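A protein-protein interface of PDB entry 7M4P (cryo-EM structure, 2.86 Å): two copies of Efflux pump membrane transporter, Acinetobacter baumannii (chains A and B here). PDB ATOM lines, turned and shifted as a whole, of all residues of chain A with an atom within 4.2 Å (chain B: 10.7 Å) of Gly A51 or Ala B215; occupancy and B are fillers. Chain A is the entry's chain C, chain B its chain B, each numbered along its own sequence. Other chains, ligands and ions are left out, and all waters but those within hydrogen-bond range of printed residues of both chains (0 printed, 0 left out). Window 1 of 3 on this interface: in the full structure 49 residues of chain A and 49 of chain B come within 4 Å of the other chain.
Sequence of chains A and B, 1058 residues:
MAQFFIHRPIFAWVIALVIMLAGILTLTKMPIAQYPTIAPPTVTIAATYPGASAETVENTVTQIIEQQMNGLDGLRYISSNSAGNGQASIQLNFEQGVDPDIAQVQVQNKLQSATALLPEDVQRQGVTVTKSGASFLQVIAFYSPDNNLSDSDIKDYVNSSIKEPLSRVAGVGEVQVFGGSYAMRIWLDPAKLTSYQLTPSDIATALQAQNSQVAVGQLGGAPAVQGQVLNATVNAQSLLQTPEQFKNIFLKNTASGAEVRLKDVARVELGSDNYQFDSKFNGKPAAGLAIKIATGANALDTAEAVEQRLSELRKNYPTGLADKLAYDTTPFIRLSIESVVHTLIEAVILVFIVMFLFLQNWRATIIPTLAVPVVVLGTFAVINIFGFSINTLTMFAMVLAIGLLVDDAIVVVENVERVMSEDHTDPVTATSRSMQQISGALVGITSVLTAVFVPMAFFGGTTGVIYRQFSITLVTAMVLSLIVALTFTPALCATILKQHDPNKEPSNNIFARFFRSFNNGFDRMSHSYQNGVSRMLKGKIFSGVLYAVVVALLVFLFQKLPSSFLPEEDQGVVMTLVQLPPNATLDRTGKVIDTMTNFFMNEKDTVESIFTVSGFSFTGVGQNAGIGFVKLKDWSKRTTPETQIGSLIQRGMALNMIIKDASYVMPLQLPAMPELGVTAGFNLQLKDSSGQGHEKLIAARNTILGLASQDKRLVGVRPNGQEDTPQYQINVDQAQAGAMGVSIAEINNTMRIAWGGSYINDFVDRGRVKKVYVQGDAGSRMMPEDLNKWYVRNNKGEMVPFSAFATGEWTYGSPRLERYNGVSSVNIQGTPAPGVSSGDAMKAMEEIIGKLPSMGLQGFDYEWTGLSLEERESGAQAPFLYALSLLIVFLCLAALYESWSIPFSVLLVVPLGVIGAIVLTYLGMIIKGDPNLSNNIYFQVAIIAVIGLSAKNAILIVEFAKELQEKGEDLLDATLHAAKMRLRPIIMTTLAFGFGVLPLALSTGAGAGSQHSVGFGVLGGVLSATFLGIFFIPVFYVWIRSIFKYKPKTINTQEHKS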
ATOM      1  N   TYR A  49      -9.454  -7.878 -19.933  1.00  0.00           N
ATOM      2  CA  TYR A  49     -10.715  -7.533 -20.588  1.00  0.00           C
ATOM      3  C   TYR A  49     -10.798  -6.015 -20.647  1.00  0.00           C
ATOM      4  O   TYR A  49     -11.446  -5.391 -19.802  1.00  0.00           O
ATOM      5  CB  TYR A  49     -11.897  -8.134 -19.828  1.00  0.00           C
ATOM      6  CG  TYR A  49     -13.255  -8.017 -20.484  1.00  0.00           C
ATOM      7  CD1 TYR A  49     -13.462  -7.225 -21.598  1.00  0.00           C
ATOM      8  CD2 TYR A  49     -14.336  -8.697 -19.966  1.00  0.00           C
ATOM      9  CE1 TYR A  49     -14.693  -7.117 -22.171  1.00  0.00           C
ATOM     10  CE2 TYR A  49     -15.575  -8.605 -20.544  1.00  0.00           C
ATOM     11  CZ  TYR A  49     -15.747  -7.812 -21.644  1.00  0.00           C
ATOM     12  OH  TYR A  49     -16.987  -7.716 -22.213  1.00  0.00           O
ATOM     13  N   PRO A  50     -10.176  -5.391 -21.643  1.00  0.00           N
ATOM     14  CA  PRO A  50     -10.021  -3.934 -21.614  1.00  0.00           C
ATOM     15  C   PRO A  50     -11.335  -3.208 -21.377  1.00  0.00           C
ATOM     16  O   PRO A  50     -12.332  -3.452 -22.051  1.00  0.00           O
ATOM     17  CB  PRO A  50      -9.446  -3.619 -22.997  1.00  0.00           C
ATOM     18  CG  PRO A  50      -8.787  -4.858 -23.412  1.00  0.00           C
ATOM     19  CD  PRO A  50      -9.619  -5.965 -22.877  1.00  0.00           C
ATOM     20  N   GLY A  51     -11.324  -2.296 -20.416  1.00  0.00           N
ATOM     21  CA  GLY A  51     -12.442  -1.417 -20.187  1.00  0.00           C
ATOM     22  C   GLY A  51     -13.490  -1.916 -19.222  1.00  0.00           C
ATOM     23  O   GLY A  51     -14.487  -1.219 -19.013  1.00  0.00           O
ATOM     24  N   ALA A  52     -13.305  -3.087 -18.627  1.00  0.00           N
ATOM     25  CA  ALA A  52     -14.342  -3.703 -17.817  1.00  0.00           C
ATOM     26  C   ALA A  52     -14.139  -3.403 -16.337  1.00  0.00           C
ATOM     27  O   ALA A  52     -13.015  -3.223 -15.865  1.00  0.00           O
ATOM     28  CB  ALA A  52     -14.368  -5.215 -18.044  1.00  0.00           C
ATOM     29  N   SER A  53     -15.250  -3.347 -15.608  1.00  0.00           N
ATOM     30  CA  SER A  53     -15.210  -3.222 -14.166  1.00  0.00           C
ATOM     31  C   SER A  53     -14.788  -4.541 -13.541  1.00  0.00           C
ATOM     32  O   SER A  53     -14.829  -5.595 -14.174  1.00  0.00           O
ATOM     33  CB  SER A  53     -16.574  -2.811 -13.621  1.00  0.00           C
ATOM     34  OG  SER A  53     -17.544  -3.808 -13.879  1.00  0.00           O
ATOM     35  N   ASN A  85      -9.121  -2.348 -13.656  1.00  0.00           N
ATOM     36  CA  ASN A  85      -8.500  -1.959 -14.908  1.00  0.00           C
ATOM     37  C   ASN A  85      -8.882  -2.908 -16.035  1.00  0.00           C
ATOM     38  O   ASN A  85      -8.866  -2.506 -17.201  1.00  0.00           O
ATOM     39  CB  ASN A  85      -6.986  -1.903 -14.745  1.00  0.00           C
ATOM     40  CG  ASN A  85      -6.409  -3.203 -14.261  1.00  0.00           C
ATOM     41  OD1 ASN A  85      -7.134  -4.108 -13.873  1.00  0.00           O
ATOM     42  ND2 ASN A  85      -5.096  -3.297 -14.263  1.00  0.00           N
ATOM     43  N   ASN A 748     -14.954   5.065 -28.572  1.00  0.00           N
ATOM     44  CA  ASN A 748     -14.018   4.192 -27.883  1.00  0.00           C
ATOM     45  C   ASN A 748     -12.604   4.430 -28.381  1.00  0.00           C
ATOM     46  O   ASN A 748     -11.680   4.638 -27.593  1.00  0.00           O
ATOM     47  CB  ASN A 748     -14.383   2.722 -28.060  1.00  0.00           C
ATOM     48  CG  ASN A 748     -13.259   1.803 -27.606  1.00  0.00           C
ATOM     49  OD1 ASN A 748     -13.086   1.550 -26.416  1.00  0.00           O
ATOM     50  ND2 ASN A 748     -12.470   1.330 -28.555  1.00  0.00           N
ATOM     51  N   ARG A 752      -9.865   6.060 -25.879  1.00  0.00           N
ATOM     52  CA  ARG A 752      -8.867   5.065 -25.523  1.00  0.00           C
ATOM     53  C   ARG A 752      -7.465   5.547 -25.850  1.00  0.00           C
ATOM     54  O   ARG A 752      -6.580   5.530 -24.992  1.00  0.00           O
ATOM     55  CB  ARG A 752      -9.192   3.778 -26.273  1.00  0.00           C
ATOM     56  CG  ARG A 752      -8.291   2.627 -26.002  1.00  0.00           C
ATOM     57  CD  ARG A 752      -8.618   1.488 -26.937  1.00  0.00           C
ATOM     58  NE  ARG A 752      -8.507   1.889 -28.330  1.00  0.00           N
ATOM     59  CZ  ARG A 752      -7.359   2.084 -28.965  1.00  0.00           C
ATOM     60  NH1 ARG A 752      -7.363   2.447 -30.235  1.00  0.00           N
ATOM     61  NH2 ARG A 752      -6.205   1.921 -28.334  1.00  0.00           N
ATOM     62  N   ASN B 211     -22.968  -0.916 -30.460  1.00  0.00           N
ATOM     63  CA  ASN B 211     -22.863  -1.764 -29.278  1.00  0.00           C
ATOM     64  C   ASN B 211     -21.389  -2.045 -29.030  1.00  0.00           C
ATOM     65  O   ASN B 211     -20.777  -2.822 -29.766  1.00  0.00           O
ATOM     66  CB  ASN B 211     -23.638  -3.062 -29.456  1.00  0.00           C
ATOM     67  CG  ASN B 211     -23.706  -3.855 -28.194  1.00  0.00           C
ATOM     68  OD1 ASN B 211     -23.065  -3.515 -27.220  1.00  0.00           O
ATOM     69  ND2 ASN B 211     -24.489  -4.914 -28.195  1.00  0.00           N
ATOM     70  N   SER B 212     -20.820  -1.435 -27.994  1.00  0.00           N
ATOM     71  CA  SER B 212     -19.393  -1.566 -27.751  1.00  0.00           C
ATOM     72  C   SER B 212     -19.090  -1.354 -26.277  1.00  0.00           C
ATOM     73  O   SER B 212     -19.915  -0.855 -25.512  1.00  0.00           O
ATOM     74  CB  SER B 212     -18.589  -0.568 -28.588  1.00  0.00           C
ATOM     75  OG  SER B 212     -19.110  -0.455 -29.900  1.00  0.00           O
ATOM     76  N   GLN B 213     -17.883  -1.744 -25.891  1.00  0.00           N
ATOM     77  CA  GLN B 213     -17.293  -1.347 -24.626  1.00  0.00           C
ATOM     78  C   GLN B 213     -16.303  -0.224 -24.883  1.00  0.00           C
ATOM     79  O   GLN B 213     -15.491  -0.314 -25.808  1.00  0.00           O
ATOM     80  CB  GLN B 213     -16.586  -2.523 -23.957  1.00  0.00           C
ATOM     81  CG  GLN B 213     -16.239  -2.286 -22.503  1.00  0.00           C
ATOM     82  CD  GLN B 213     -17.444  -1.842 -21.686  1.00  0.00           C
ATOM     83  OE1 GLN B 213     -17.552  -0.680 -21.296  1.00  0.00           O
ATOM     84  NE2 GLN B 213     -18.363  -2.764 -21.444  1.00  0.00           N
ATOM     85  N   VAL B 214     -16.359   0.822 -24.068  1.00  0.00           N
ATOM     86  CA  VAL B 214     -15.452   1.957 -24.188  1.00  0.00           C
ATOM     87  C   VAL B 214     -14.394   1.854 -23.099  1.00  0.00           C
ATOM     88  O   VAL B 214     -14.712   1.916 -21.908  1.00  0.00           O
ATOM     89  CB  VAL B 214     -16.204   3.293 -24.091  1.00  0.00           C
ATOM     90  CG1 VAL B 214     -15.243   4.441 -24.304  1.00  0.00           C
ATOM     91  CG2 VAL B 214     -17.340   3.357 -25.099  1.00  0.00           C
ATOM     92  N   ALA B 215     -13.135   1.695 -23.496  1.00  0.00           N
ATOM     93  CA  ALA B 215     -12.013   1.836 -22.577  1.00  0.00           C
ATOM     94  C   ALA B 215     -11.558   3.287 -22.558  1.00  0.00           C
ATOM     95  O   ALA B 215     -11.616   3.975 -23.578  1.00  0.00           O
ATOM     96  CB  ALA B 215     -10.856   0.927 -22.981  1.00  0.00           C
ATOM     97  N   VAL B 216     -11.139   3.765 -21.387  1.00  0.00           N
ATOM     98  CA  VAL B 216     -10.769   5.170 -21.237  1.00  0.00           C
ATOM     99  C   VAL B 216      -9.340   5.309 -20.727  1.00  0.00           C
ATOM    100  O   VAL B 216      -8.452   5.736 -21.464  1.00  0.00           O
ATOM    101  CB  VAL B 216     -11.757   5.887 -20.299  1.00  0.00           C
ATOM    102  CG1 VAL B 216     -11.428   7.366 -20.170  1.00  0.00           C
ATOM    103  CG2 VAL B 216     -13.161   5.723 -20.816  1.00  0.00           C
ATOM    104  N   GLY B 217      -9.096   4.908 -19.483  1.00  0.00           N
ATOM    105  CA  GLY B 217      -7.802   5.124 -18.862  1.00  0.00           C
ATOM    106  C   GLY B 217      -7.860   5.455 -17.387  1.00  0.00           C
ATOM    107  O   GLY B 217      -8.441   4.714 -16.592  1.00  0.00           O
ATOM    108  N   GLN B 218      -7.244   6.565 -17.002  1.00  0.00           N
ATOM    109  CA  GLN B 218      -7.122   6.923 -15.599  1.00  0.00           C
ATOM    110  C   GLN B 218      -7.060   8.434 -15.453  1.00  0.00           C
ATOM    111  O   GLN B 218      -6.620   9.140 -16.358  1.00  0.00           O
ATOM    112  CB  GLN B 218      -5.873   6.297 -14.986  1.00  0.00           C
ATOM    113  CG  GLN B 218      -6.149   5.143 -14.088  1.00  0.00           C
ATOM    114  CD  GLN B 218      -4.904   4.437 -13.680  1.00  0.00           C
ATOM    115  OE1 GLN B 218      -3.865   4.606 -14.289  1.00  0.00           O
ATOM    116  NE2 GLN B 218      -4.998   3.621 -12.646  1.00  0.00           N
ATOM    117  N   THR B 233      -9.531   5.580 -11.600  1.00  0.00           N
ATOM    118  CA  THR B 233      -9.802   4.839 -12.824  1.00  0.00           C
ATOM    119  C   THR B 233     -11.115   5.311 -13.428  1.00  0.00           C
ATOM    120  O   THR B 233     -12.108   5.466 -12.717  1.00  0.00           O
ATOM    121  CB  THR B 233      -9.869   3.341 -12.543  1.00  0.00           C
ATOM    122  OG1 THR B 233      -8.675   2.927 -11.883  1.00  0.00           O
ATOM    123  CG2 THR B 233     -10.010   2.561 -13.820  1.00  0.00           C
ATOM    124  N   VAL B 234     -11.115   5.549 -14.733  1.00  0.00           N
ATOM    125  CA  VAL B 234     -12.310   5.968 -15.452  1.00  0.00           C
ATOM    126  C   VAL B 234     -12.848   4.759 -16.197  1.00  0.00           C
ATOM    127  O   VAL B 234     -12.207   4.260 -17.125  1.00  0.00           O
ATOM    128  CB  VAL B 234     -12.021   7.122 -16.417  1.00  0.00           C
ATOM    129  CG1 VAL B 234     -13.332   7.782 -16.844  1.00  0.00           C
ATOM    130  CG2 VAL B 234     -11.072   8.129 -15.792  1.00  0.00           C
ATOM    131  N   ASN B 235     -14.038   4.301 -15.804  1.00  0.00           N
ATOM    132  CA  ASN B 235     -14.750   3.228 -16.487  1.00  0.00           C
ATOM    133  C   ASN B 235     -16.025   3.764 -17.132  1.00  0.00           C
ATOM    134  O   ASN B 235     -16.747   4.560 -16.528  1.00  0.00           O
ATOM    135  CB  ASN B 235     -15.089   2.097 -15.515  1.00  0.00           C
ATOM    136  CG  ASN B 235     -14.089   0.953 -15.571  1.00  0.00           C
ATOM    137  OD1 ASN B 235     -13.260   0.877 -16.475  1.00  0.00           O
ATOM    138  ND2 ASN B 235     -14.176   0.046 -14.603  1.00  0.00           N
ATOM    139  N   ALA B 236     -16.302   3.322 -18.357  1.00  0.00           N
ATOM    140  CA  ALA B 236     -17.438   3.797 -19.145  1.00  0.00           C
ATOM    141  C   ALA B 236     -18.318   2.620 -19.545  1.00  0.00           C
ATOM    142  O   ALA B 236     -17.929   1.813 -20.395  1.00  0.00           O
ATOM    143  CB  ALA B 236     -16.955   4.546 -20.386  1.00  0.00           C
ATOM    144  N   GLN B 237     -19.514   2.538 -18.967  1.00  0.00           N
ATOM    145  CA  GLN B 237     -20.436   1.450 -19.280  1.00  0.00           C
ATOM    146  C   GLN B 237     -21.234   1.791 -20.538  1.00  0.00           C
ATOM    147  O   GLN B 237     -21.999   2.762 -20.553  1.00  0.00           O
ATOM    148  CB  GLN B 237     -21.363   1.183 -18.098  1.00  0.00           C
ATOM    149  CG  GLN B 237     -22.289   2.327 -17.738  1.00  0.00           C
ATOM    150  CD  GLN B 237     -23.019   2.086 -16.433  1.00  0.00           C
ATOM    151  OE1 GLN B 237     -22.825   1.059 -15.783  1.00  0.00           O
ATOM    152  NE2 GLN B 237     -23.865   3.032 -16.043  1.00  0.00           N
ATOM    153  N   SER B 238     -21.050   0.998 -21.598  1.00  0.00           N
ATOM    154  CA  SER B 238     -21.636   1.322 -22.893  1.00  0.00           C
ATOM    155  C   SER B 238     -22.426   0.170 -23.497  1.00  0.00           C
ATOM    156  O   SER B 238     -23.403   0.397 -24.214  1.00  0.00           O
ATOM    157  CB  SER B 238     -20.545   1.745 -23.869  1.00  0.00           C
ATOM    158  OG  SER B 238     -19.930   2.935 -23.443  1.00  0.00           O
ATOM    159  N   LEU B 239     -22.021  -1.067 -23.219  1.00  0.00           N
ATOM    160  CA  LEU B 239     -22.677  -2.209 -23.834  1.00  0.00           C
ATOM    161  C   LEU B 239     -24.163  -2.195 -23.524  1.00  0.00           C
ATOM    162  O   LEU B 239     -24.597  -1.713 -22.475  1.00  0.00           O
ATOM    163  CB  LEU B 239     -22.065  -3.516 -23.340  1.00  0.00           C
ATOM    164  CG  LEU B 239     -20.792  -4.021 -24.017  1.00  0.00           C
ATOM    165  CD1 LEU B 239     -20.305  -5.251 -23.316  1.00  0.00           C
ATOM    166  CD2 LEU B 239     -21.035  -4.325 -25.461  1.00  0.00           C
ATOM    167  N   VAL B 764     -23.738  -8.138 -22.484  1.00  0.00           N
ATOM    168  CA  VAL B 764     -23.688  -8.803 -21.190  1.00  0.00           C
ATOM    169  C   VAL B 764     -25.041  -8.840 -20.536  1.00  0.00           C
ATOM    170  O   VAL B 764     -25.421  -7.884 -19.922  1.00  0.00           O
ATOM    171  CB  VAL B 764     -22.718  -8.104 -20.226  1.00  0.00           C
ATOM    172  CG1 VAL B 764     -21.295  -8.560 -20.495  1.00  0.00           C
ATOM    173  CG2 VAL B 764     -22.822  -6.593 -20.352  1.00  0.00           C
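The backbone NH of Ala B215 is in hydrogen-bond range of the side-chain amide oxygen of Asn A748, 2.9 Å away.
O of Gln B213 sits close to OD1 of Asn A748.
O of Ala B236 lies close to OE1 of Gln B213, at 2.7 Å.
No position is printed for both chains.
Of the 10 pairs that touch across the chains among the printed residues, none has its exchanged pair printed and touching as well.
Among the printed residues, merely in contact across the chains: Gly A51 with Gln B213 (3.9 Å), Gly A51 with Ala B215 (3.98 Å), Gly A51 with Asn B235 (3.5 Å), Ala A52 with Asn B235 (3.7 Å), Ser A53 with Asn B235 (3.5 Å), Asn A748 with Val B214 (3.3 Å), Arg A752 with Ala B215 (3.5 Å) and Arg A752 with Val B216 (3.999 Å).
Along chain B the printed residues that touch a printed residue of chain A span positions 213 to 235.
Of the 8 printed residues of chain A, 5 touch a printed residue of chain B.
Printed residues of chain A that touch a printed residue of chain B: Gly A51, Ala A52, Ser A53, Asn A748 and Arg A752.
Among the printed residues, no Asp or Glu carboxylate lies within 4 Å of a Lys or Arg side-chain nitrogen of the other chain.
No residue of chain B comes within 4 Å of Pro A50.
Gly A51 touches three residues of chain B.
Of chain B, only Asn B235 (3.7 Å) comes within 4 Å of Ala A52.
Asn A85 touches none of the printed residues of chain B.
Of chain B, only Gln B213, Val B214 and Ala B215 come within 4 Å of Asn A748.
Of the printed residues of chain B, Arg A752 touches Ala B215 (3.5 Å) and Val B216 (3.999 Å).
Of the printed residues of chain A, Gln B213 touches Gly A51 and Asn A748.
Of the printed residues of chain A, Val B214 touches Asn A748.
Printed residues of chain A within 4 Å of Val B216: Arg A752 (3.999 Å).
The nearest printed residue of chain A that does not touch Val B214 is Gly A51 (4.3 Å).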
